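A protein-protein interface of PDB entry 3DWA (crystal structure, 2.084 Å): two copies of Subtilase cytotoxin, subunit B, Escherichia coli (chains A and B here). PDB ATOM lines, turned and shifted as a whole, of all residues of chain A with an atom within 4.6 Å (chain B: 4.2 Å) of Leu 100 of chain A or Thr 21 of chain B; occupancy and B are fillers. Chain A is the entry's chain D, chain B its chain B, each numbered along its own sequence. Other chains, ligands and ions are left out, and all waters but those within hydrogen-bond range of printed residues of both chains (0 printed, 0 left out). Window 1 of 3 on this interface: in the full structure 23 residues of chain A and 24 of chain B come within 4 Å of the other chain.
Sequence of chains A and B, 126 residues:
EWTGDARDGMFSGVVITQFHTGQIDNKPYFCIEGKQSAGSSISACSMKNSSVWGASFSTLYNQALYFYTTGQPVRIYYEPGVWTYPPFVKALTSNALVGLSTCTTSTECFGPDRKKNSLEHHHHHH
The backbone NH (N) of Arg 75 of chain A is in hydrogen-bond range of the backbone carbonyl oxygen (O) of Ser 101 of chain A, at 2.7 Å.
N of Tyr 77 of chain A sits at hydrogen-bond distance from O of Gly 99 of chain A, at 3.2 Å.
No position is printed for both chains.
The backbone NH of Thr 21 of chain B is in hydrogen-bond range of the backbone carbonyl oxygen of Leu 100 of chain A (2.8 Å).
Thr 21 of chain B touches Thr 59 of chain A.
Leu 60 of chain A touches Thr 21 of chain B.
CE2 of Tyr 77 of chain A touches CD2 of His 20 of chain B, 3.8 Å away.
Gly 99 of chain A touches Thr 21 of chain B.
His 20 of chain B touches Leu 100 of chain A.
His 20 of chain B touches Ser 101 of chain A (CD2 to OG, 2.8 Å).
Along chain A the printed residues that touch a printed residue of chain B span positions 59 to 101.
Of the 5 printed residues of chain B, 2 touch a printed residue of chain A.
Hydrophobic or aromatic side chains of chain B that line the printed part of chain A: His 20.
Among the printed residues, 7 pairs touch across the chains.
Of chain B, only His 20 and Thr 21 come within 4 Å of Leu 100 of chain A.
Of the printed residues of chain A, Thr 21 of chain B touches Thr 59 (3.3 Å), Leu 60 (3.6 Å), Gly 99 (3.1 Å) and Leu 100 (2.8 Å).
Of the printed residues of chain B, Leu 60 of chain A touches Thr 21.
Of the printed residues of chain B, Thr 59 of chain A touches Thr 21 (3.3 Å).
Ile 16 of chain A touches none of the printed residues of chain B.
The nearest residue of chain A that does not touch Thr 21 of chain B is Gln 63 of chain A (4.3 Å).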
ATOM      1  N   ILE A  16      -2.278  -2.908  -4.837  1.00  0.00           N
ATOM      2  CA  ILE A  16      -3.154  -1.776  -5.184  1.00  0.00           C
ATOM      3  C   ILE A  16      -4.253  -2.285  -6.122  1.00  0.00           C
ATOM      4  O   ILE A  16      -3.979  -2.753  -7.265  1.00  0.00           O
ATOM      5  CB  ILE A  16      -2.359  -0.603  -5.800  1.00  0.00           C
ATOM      6  CG1 ILE A  16      -1.308  -0.089  -4.784  1.00  0.00           C
ATOM      7  CG2 ILE A  16      -3.298   0.502  -6.276  1.00  0.00           C
ATOM      8  CD1 ILE A  16      -0.311   0.818  -5.406  1.00  0.00           C
ATOM      9  N   ILE A  32      -5.842   5.842  -4.251  1.00  0.00           N
ATOM     10  CA  ILE A  32      -5.685   4.415  -4.448  1.00  0.00           C
ATOM     11  C   ILE A  32      -6.208   3.682  -3.225  1.00  0.00           C
ATOM     12  O   ILE A  32      -6.243   4.241  -2.134  1.00  0.00           O
ATOM     13  CB  ILE A  32      -4.217   4.018  -4.707  1.00  0.00           C
ATOM     14  CG1 ILE A  32      -3.287   4.670  -3.646  1.00  0.00           C
ATOM     15  CG2 ILE A  32      -3.797   4.420  -6.130  1.00  0.00           C
ATOM     16  CD1 ILE A  32      -1.798   4.278  -3.806  1.00  0.00           C
ATOM     17  N   THR A  59       5.192  12.041  -9.718  1.00  0.00           N
ATOM     18  CA  THR A  59       5.974  10.836  -9.381  1.00  0.00           C
ATOM     19  C   THR A  59       5.126   9.749  -8.751  1.00  0.00           C
ATOM     20  O   THR A  59       5.239   8.588  -9.148  1.00  0.00           O
ATOM     21  CB  THR A  59       7.180  11.167  -8.400  1.00  0.00           C
ATOM     22  OG1 THR A  59       7.978  12.180  -8.988  1.00  0.00           O
ATOM     23  CG2 THR A  59       8.083   9.953  -8.134  1.00  0.00           C
ATOM     24  N   LEU A  60       4.298  10.120  -7.775  1.00  0.00           N
ATOM     25  CA  LEU A  60       3.411   9.161  -7.095  1.00  0.00           C
ATOM     26  C   LEU A  60       2.311   8.590  -8.047  1.00  0.00           C
ATOM     27  O   LEU A  60       1.993   7.376  -8.013  1.00  0.00           O
ATOM     28  CB  LEU A  60       2.784   9.807  -5.849  1.00  0.00           C
ATOM     29  CG  LEU A  60       3.721  10.018  -4.634  1.00  0.00           C
ATOM     30  CD1 LEU A  60       3.051  10.875  -3.558  1.00  0.00           C
ATOM     31  CD2 LEU A  60       4.244   8.711  -4.027  1.00  0.00           C
ATOM     32  N   GLN A  63       4.025   6.097 -10.375  1.00  0.00           N
ATOM     33  CA  GLN A  63       4.481   4.928  -9.663  1.00  0.00           C
ATOM     34  C   GLN A  63       3.284   4.098  -9.158  1.00  0.00           C
ATOM     35  O   GLN A  63       3.299   2.850  -9.237  1.00  0.00           O
ATOM     36  CB  GLN A  63       5.443   5.306  -8.504  1.00  0.00           C
ATOM     37  CG  GLN A  63       6.191   4.097  -7.904  1.00  0.00           C
ATOM     38  CD  GLN A  63       7.223   3.558  -8.895  1.00  0.00           C
ATOM     39  OE1 GLN A  63       7.913   4.318  -9.535  1.00  0.00           O
ATOM     40  NE2 GLN A  63       7.265   2.262  -9.064  1.00  0.00           N
ATOM     41  N   ALA A  64       2.244   4.774  -8.680  1.00  0.00           N
ATOM     42  CA  ALA A  64       0.991   4.093  -8.275  1.00  0.00           C
ATOM     43  C   ALA A  64       0.309   3.373  -9.458  1.00  0.00           C
ATOM     44  O   ALA A  64      -0.074   2.240  -9.311  1.00  0.00           O
ATOM     45  CB  ALA A  64      -0.013   5.066  -7.616  1.00  0.00           C
ATOM     46  N   PHE A  67       2.367   0.214 -10.301  1.00  0.00           N
ATOM     47  CA  PHE A  67       2.103  -0.853  -9.365  1.00  0.00           C
ATOM     48  C   PHE A  67       0.699  -1.417  -9.477  1.00  0.00           C
ATOM     49  O   PHE A  67       0.490  -2.637  -9.215  1.00  0.00           O
ATOM     50  CB  PHE A  67       2.368  -0.416  -7.915  1.00  0.00           C
ATOM     51  CG  PHE A  67       3.858  -0.197  -7.564  1.00  0.00           C
ATOM     52  CD1 PHE A  67       4.845  -1.080  -7.998  1.00  0.00           C
ATOM     53  CD2 PHE A  67       4.247   0.885  -6.750  1.00  0.00           C
ATOM     54  CE1 PHE A  67       6.211  -0.892  -7.659  1.00  0.00           C
ATOM     55  CE2 PHE A  67       5.606   1.059  -6.391  1.00  0.00           C
ATOM     56  CZ  PHE A  67       6.578   0.170  -6.868  1.00  0.00           C
ATOM     57  N   ARG A  75       4.539  -1.191  -0.428  1.00  0.00           N
ATOM     58  CA  ARG A  75       4.303  -0.482   0.810  1.00  0.00           C
ATOM     59  C   ARG A  75       3.674   0.865   0.494  1.00  0.00           C
ATOM     60  O   ARG A  75       4.196   1.575  -0.381  1.00  0.00           O
ATOM     61  CB  ARG A  75       5.637  -0.279   1.557  1.00  0.00           C
ATOM     62  CG  ARG A  75       5.538   0.621   2.783  1.00  0.00           C
ATOM     63  CD  ARG A  75       6.888   0.582   3.475  1.00  0.00           C
ATOM     64  NE  ARG A  75       7.073  -0.674   4.239  1.00  0.00           N
ATOM     65  CZ  ARG A  75       8.215  -1.032   4.841  1.00  0.00           C
ATOM     66  NH1 ARG A  75       9.295  -0.250   4.765  1.00  0.00           N
ATOM     67  NH2 ARG A  75       8.287  -2.184   5.506  1.00  0.00           N
ATOM     68  N   ILE A  76       2.582   1.200   1.202  1.00  0.00           N
ATOM     69  CA  ILE A  76       1.956   2.524   1.116  1.00  0.00           C
ATOM     70  C   ILE A  76       2.370   3.326   2.330  1.00  0.00           C
ATOM     71  O   ILE A  76       2.093   2.937   3.478  1.00  0.00           O
ATOM     72  CB  ILE A  76       0.396   2.471   1.076  1.00  0.00           C
ATOM     73  CG1 ILE A  76      -0.141   1.677  -0.132  1.00  0.00           C
ATOM     74  CG2 ILE A  76      -0.234   3.870   1.119  1.00  0.00           C
ATOM     75  CD1 ILE A  76       0.307   2.163  -1.481  1.00  0.00           C
ATOM     76  N   TYR A  77       3.060   4.427   2.072  1.00  0.00           N
ATOM     77  CA  TYR A  77       3.343   5.413   3.099  1.00  0.00           C
ATOM     78  C   TYR A  77       2.281   6.498   3.055  1.00  0.00           C
ATOM     79  O   TYR A  77       2.031   7.090   2.009  1.00  0.00           O
ATOM     80  CB  TYR A  77       4.667   6.114   2.806  1.00  0.00           C
ATOM     81  CG  TYR A  77       5.864   5.251   2.903  1.00  0.00           C
ATOM     82  CD1 TYR A  77       6.554   5.139   4.093  1.00  0.00           C
ATOM     83  CD2 TYR A  77       6.369   4.599   1.766  1.00  0.00           C
ATOM     84  CE1 TYR A  77       7.702   4.347   4.181  1.00  0.00           C
ATOM     85  CE2 TYR A  77       7.500   3.819   1.836  1.00  0.00           C
ATOM     86  CZ  TYR A  77       8.170   3.703   3.062  1.00  0.00           C
ATOM     87  OH  TYR A  77       9.316   2.940   3.138  1.00  0.00           O
ATOM     88  N   LEU A  97      -1.074  10.392   0.392  1.00  0.00           N
ATOM     89  CA  LEU A  97      -0.076   9.406  -0.074  1.00  0.00           C
ATOM     90  C   LEU A  97       1.235  10.122  -0.079  1.00  0.00           C
ATOM     91  O   LEU A  97       1.310  11.187  -0.676  1.00  0.00           O
ATOM     92  CB  LEU A  97      -0.383   8.958  -1.533  1.00  0.00           C
ATOM     93  CG  LEU A  97       0.567   7.904  -2.115  1.00  0.00           C
ATOM     94  CD1 LEU A  97       0.587   6.633  -1.253  1.00  0.00           C
ATOM     95  CD2 LEU A  97       0.184   7.579  -3.570  1.00  0.00           C
ATOM     96  N   GLY A  99       4.593   8.247  -0.175  1.00  0.00           N
ATOM     97  CA  GLY A  99       5.670   7.486  -0.791  1.00  0.00           C
ATOM     98  C   GLY A  99       5.164   6.113  -1.088  1.00  0.00           C
ATOM     99  O   GLY A  99       4.051   5.807  -0.684  1.00  0.00           O
ATOM    100  N   LEU A 100       5.975   5.301  -1.781  1.00  0.00           N
ATOM    101  CA  LEU A 100       5.667   3.919  -2.201  1.00  0.00           C
ATOM    102  C   LEU A 100       6.961   3.113  -2.288  1.00  0.00           C
ATOM    103  O   LEU A 100       8.018   3.666  -2.652  1.00  0.00           O
ATOM    104  CB  LEU A 100       5.004   3.908  -3.614  1.00  0.00           C
ATOM    105  CG  LEU A 100       3.554   4.424  -3.828  1.00  0.00           C
ATOM    106  CD1 LEU A 100       3.277   4.740  -5.362  1.00  0.00           C
ATOM    107  CD2 LEU A 100       2.544   3.424  -3.265  1.00  0.00           C
ATOM    108  N   SER A 101       6.883   1.810  -1.997  1.00  0.00           N
ATOM    109  CA  SER A 101       8.038   0.900  -2.097  1.00  0.00           C
ATOM    110  C   SER A 101       7.638  -0.473  -2.568  1.00  0.00           C
ATOM    111  O   SER A 101       6.548  -0.930  -2.268  1.00  0.00           O
ATOM    112  CB  SER A 101       8.652   0.666  -0.696  1.00  0.00           C
ATOM    113  OG  SER A 101       9.377   1.784  -0.237  1.00  0.00           O
ATOM    114  N   HIS B  20      11.959   2.546  -4.629  1.00  0.00           N
ATOM    115  CA  HIS B  20      11.258   3.332  -3.585  1.00  0.00           C
ATOM    116  C   HIS B  20      11.099   4.762  -4.089  1.00  0.00           C
ATOM    117  O   HIS B  20      11.944   5.277  -4.781  1.00  0.00           O
ATOM    118  CB  HIS B  20      12.003   3.335  -2.218  1.00  0.00           C
ATOM    119  CG  HIS B  20      11.491   4.361  -1.239  1.00  0.00           C
ATOM    120  ND1 HIS B  20      12.233   5.469  -0.854  1.00  0.00           N
ATOM    121  CD2 HIS B  20      10.326   4.437  -0.553  1.00  0.00           C
ATOM    122  CE1 HIS B  20      11.521   6.206  -0.025  1.00  0.00           C
ATOM    123  NE2 HIS B  20      10.366   5.593   0.185  1.00  0.00           N
ATOM    124  N   THR B  21       9.962   5.353  -3.767  1.00  0.00           N
ATOM    125  CA  THR B  21       9.671   6.697  -4.147  1.00  0.00           C
ATOM    126  C   THR B  21       9.180   7.414  -2.873  1.00  0.00           C
ATOM    127  O   THR B  21       8.435   6.850  -2.091  1.00  0.00           O
ATOM    128  CB  THR B  21       8.637   6.647  -5.316  1.00  0.00           C
ATOM    129  OG1 THR B  21       9.148   7.297  -6.458  1.00  0.00           O
ATOM    130  CG2 THR B  21       7.298   7.089  -5.010  1.00  0.00           C
ATOM    131  N   GLY B  22       9.626   8.639  -2.674  1.00  0.00           N
ATOM    132  CA  GLY B  22       9.089   9.451  -1.623  1.00  0.00           C
ATOM    133  C   GLY B  22       9.408  10.909  -1.852  1.00  0.00           C
ATOM    134  O   GLY B  22       9.626  11.314  -2.986  1.00  0.00           O
ATOM    135  N   TYR B  29      11.812  12.155  -4.727  1.00  0.00           N
ATOM    136  CA  TYR B  29      13.068  11.477  -5.092  1.00  0.00           C
ATOM    137  C   TYR B  29      12.678   9.991  -5.343  1.00  0.00           C
ATOM    138  O   TYR B  29      11.616   9.590  -4.882  1.00  0.00           O
ATOM    139  CB  TYR B  29      14.070  11.587  -3.890  1.00  0.00           C
ATOM    140  CG  TYR B  29      13.612  10.821  -2.651  1.00  0.00           C
ATOM    141  CD1 TYR B  29      13.897   9.471  -2.499  1.00  0.00           C
ATOM    142  CD2 TYR B  29      12.871  11.462  -1.651  1.00  0.00           C
ATOM    143  CE1 TYR B  29      13.439   8.749  -1.375  1.00  0.00           C
ATOM    144  CE2 TYR B  29      12.439  10.770  -0.527  1.00  0.00           C
ATOM    145  CZ  TYR B  29      12.710   9.429  -0.401  1.00  0.00           C
ATOM    146  OH  TYR B  29      12.236   8.772   0.688  1.00  0.00           O
ATOM    147  N   PHE B  30      13.523   9.187  -5.993  1.00  0.00           N
ATOM    148  CA  PHE B  30      13.354   7.735  -5.964  1.00  0.00           C
ATOM    149  C   PHE B  30      14.681   7.106  -5.581  1.00  0.00           C
ATOM    150  O   PHE B  30      15.748   7.729  -5.715  1.00  0.00           O
ATOM    151  CB  PHE B  30      12.855   7.144  -7.307  1.00  0.00           C
ATOM    152  CG  PHE B  30      13.858   7.229  -8.406  1.00  0.00           C
ATOM    153  CD1 PHE B  30      14.604   6.107  -8.788  1.00  0.00           C
ATOM    154  CD2 PHE B  30      14.074   8.456  -9.067  1.00  0.00           C
ATOM    155  CE1 PHE B  30      15.542   6.221  -9.796  1.00  0.00           C
ATOM    156  CE2 PHE B  30      14.981   8.575 -10.075  1.00  0.00           C
ATOM    157  CZ  PHE B  30      15.751   7.448 -10.444  1.00  0.00           C
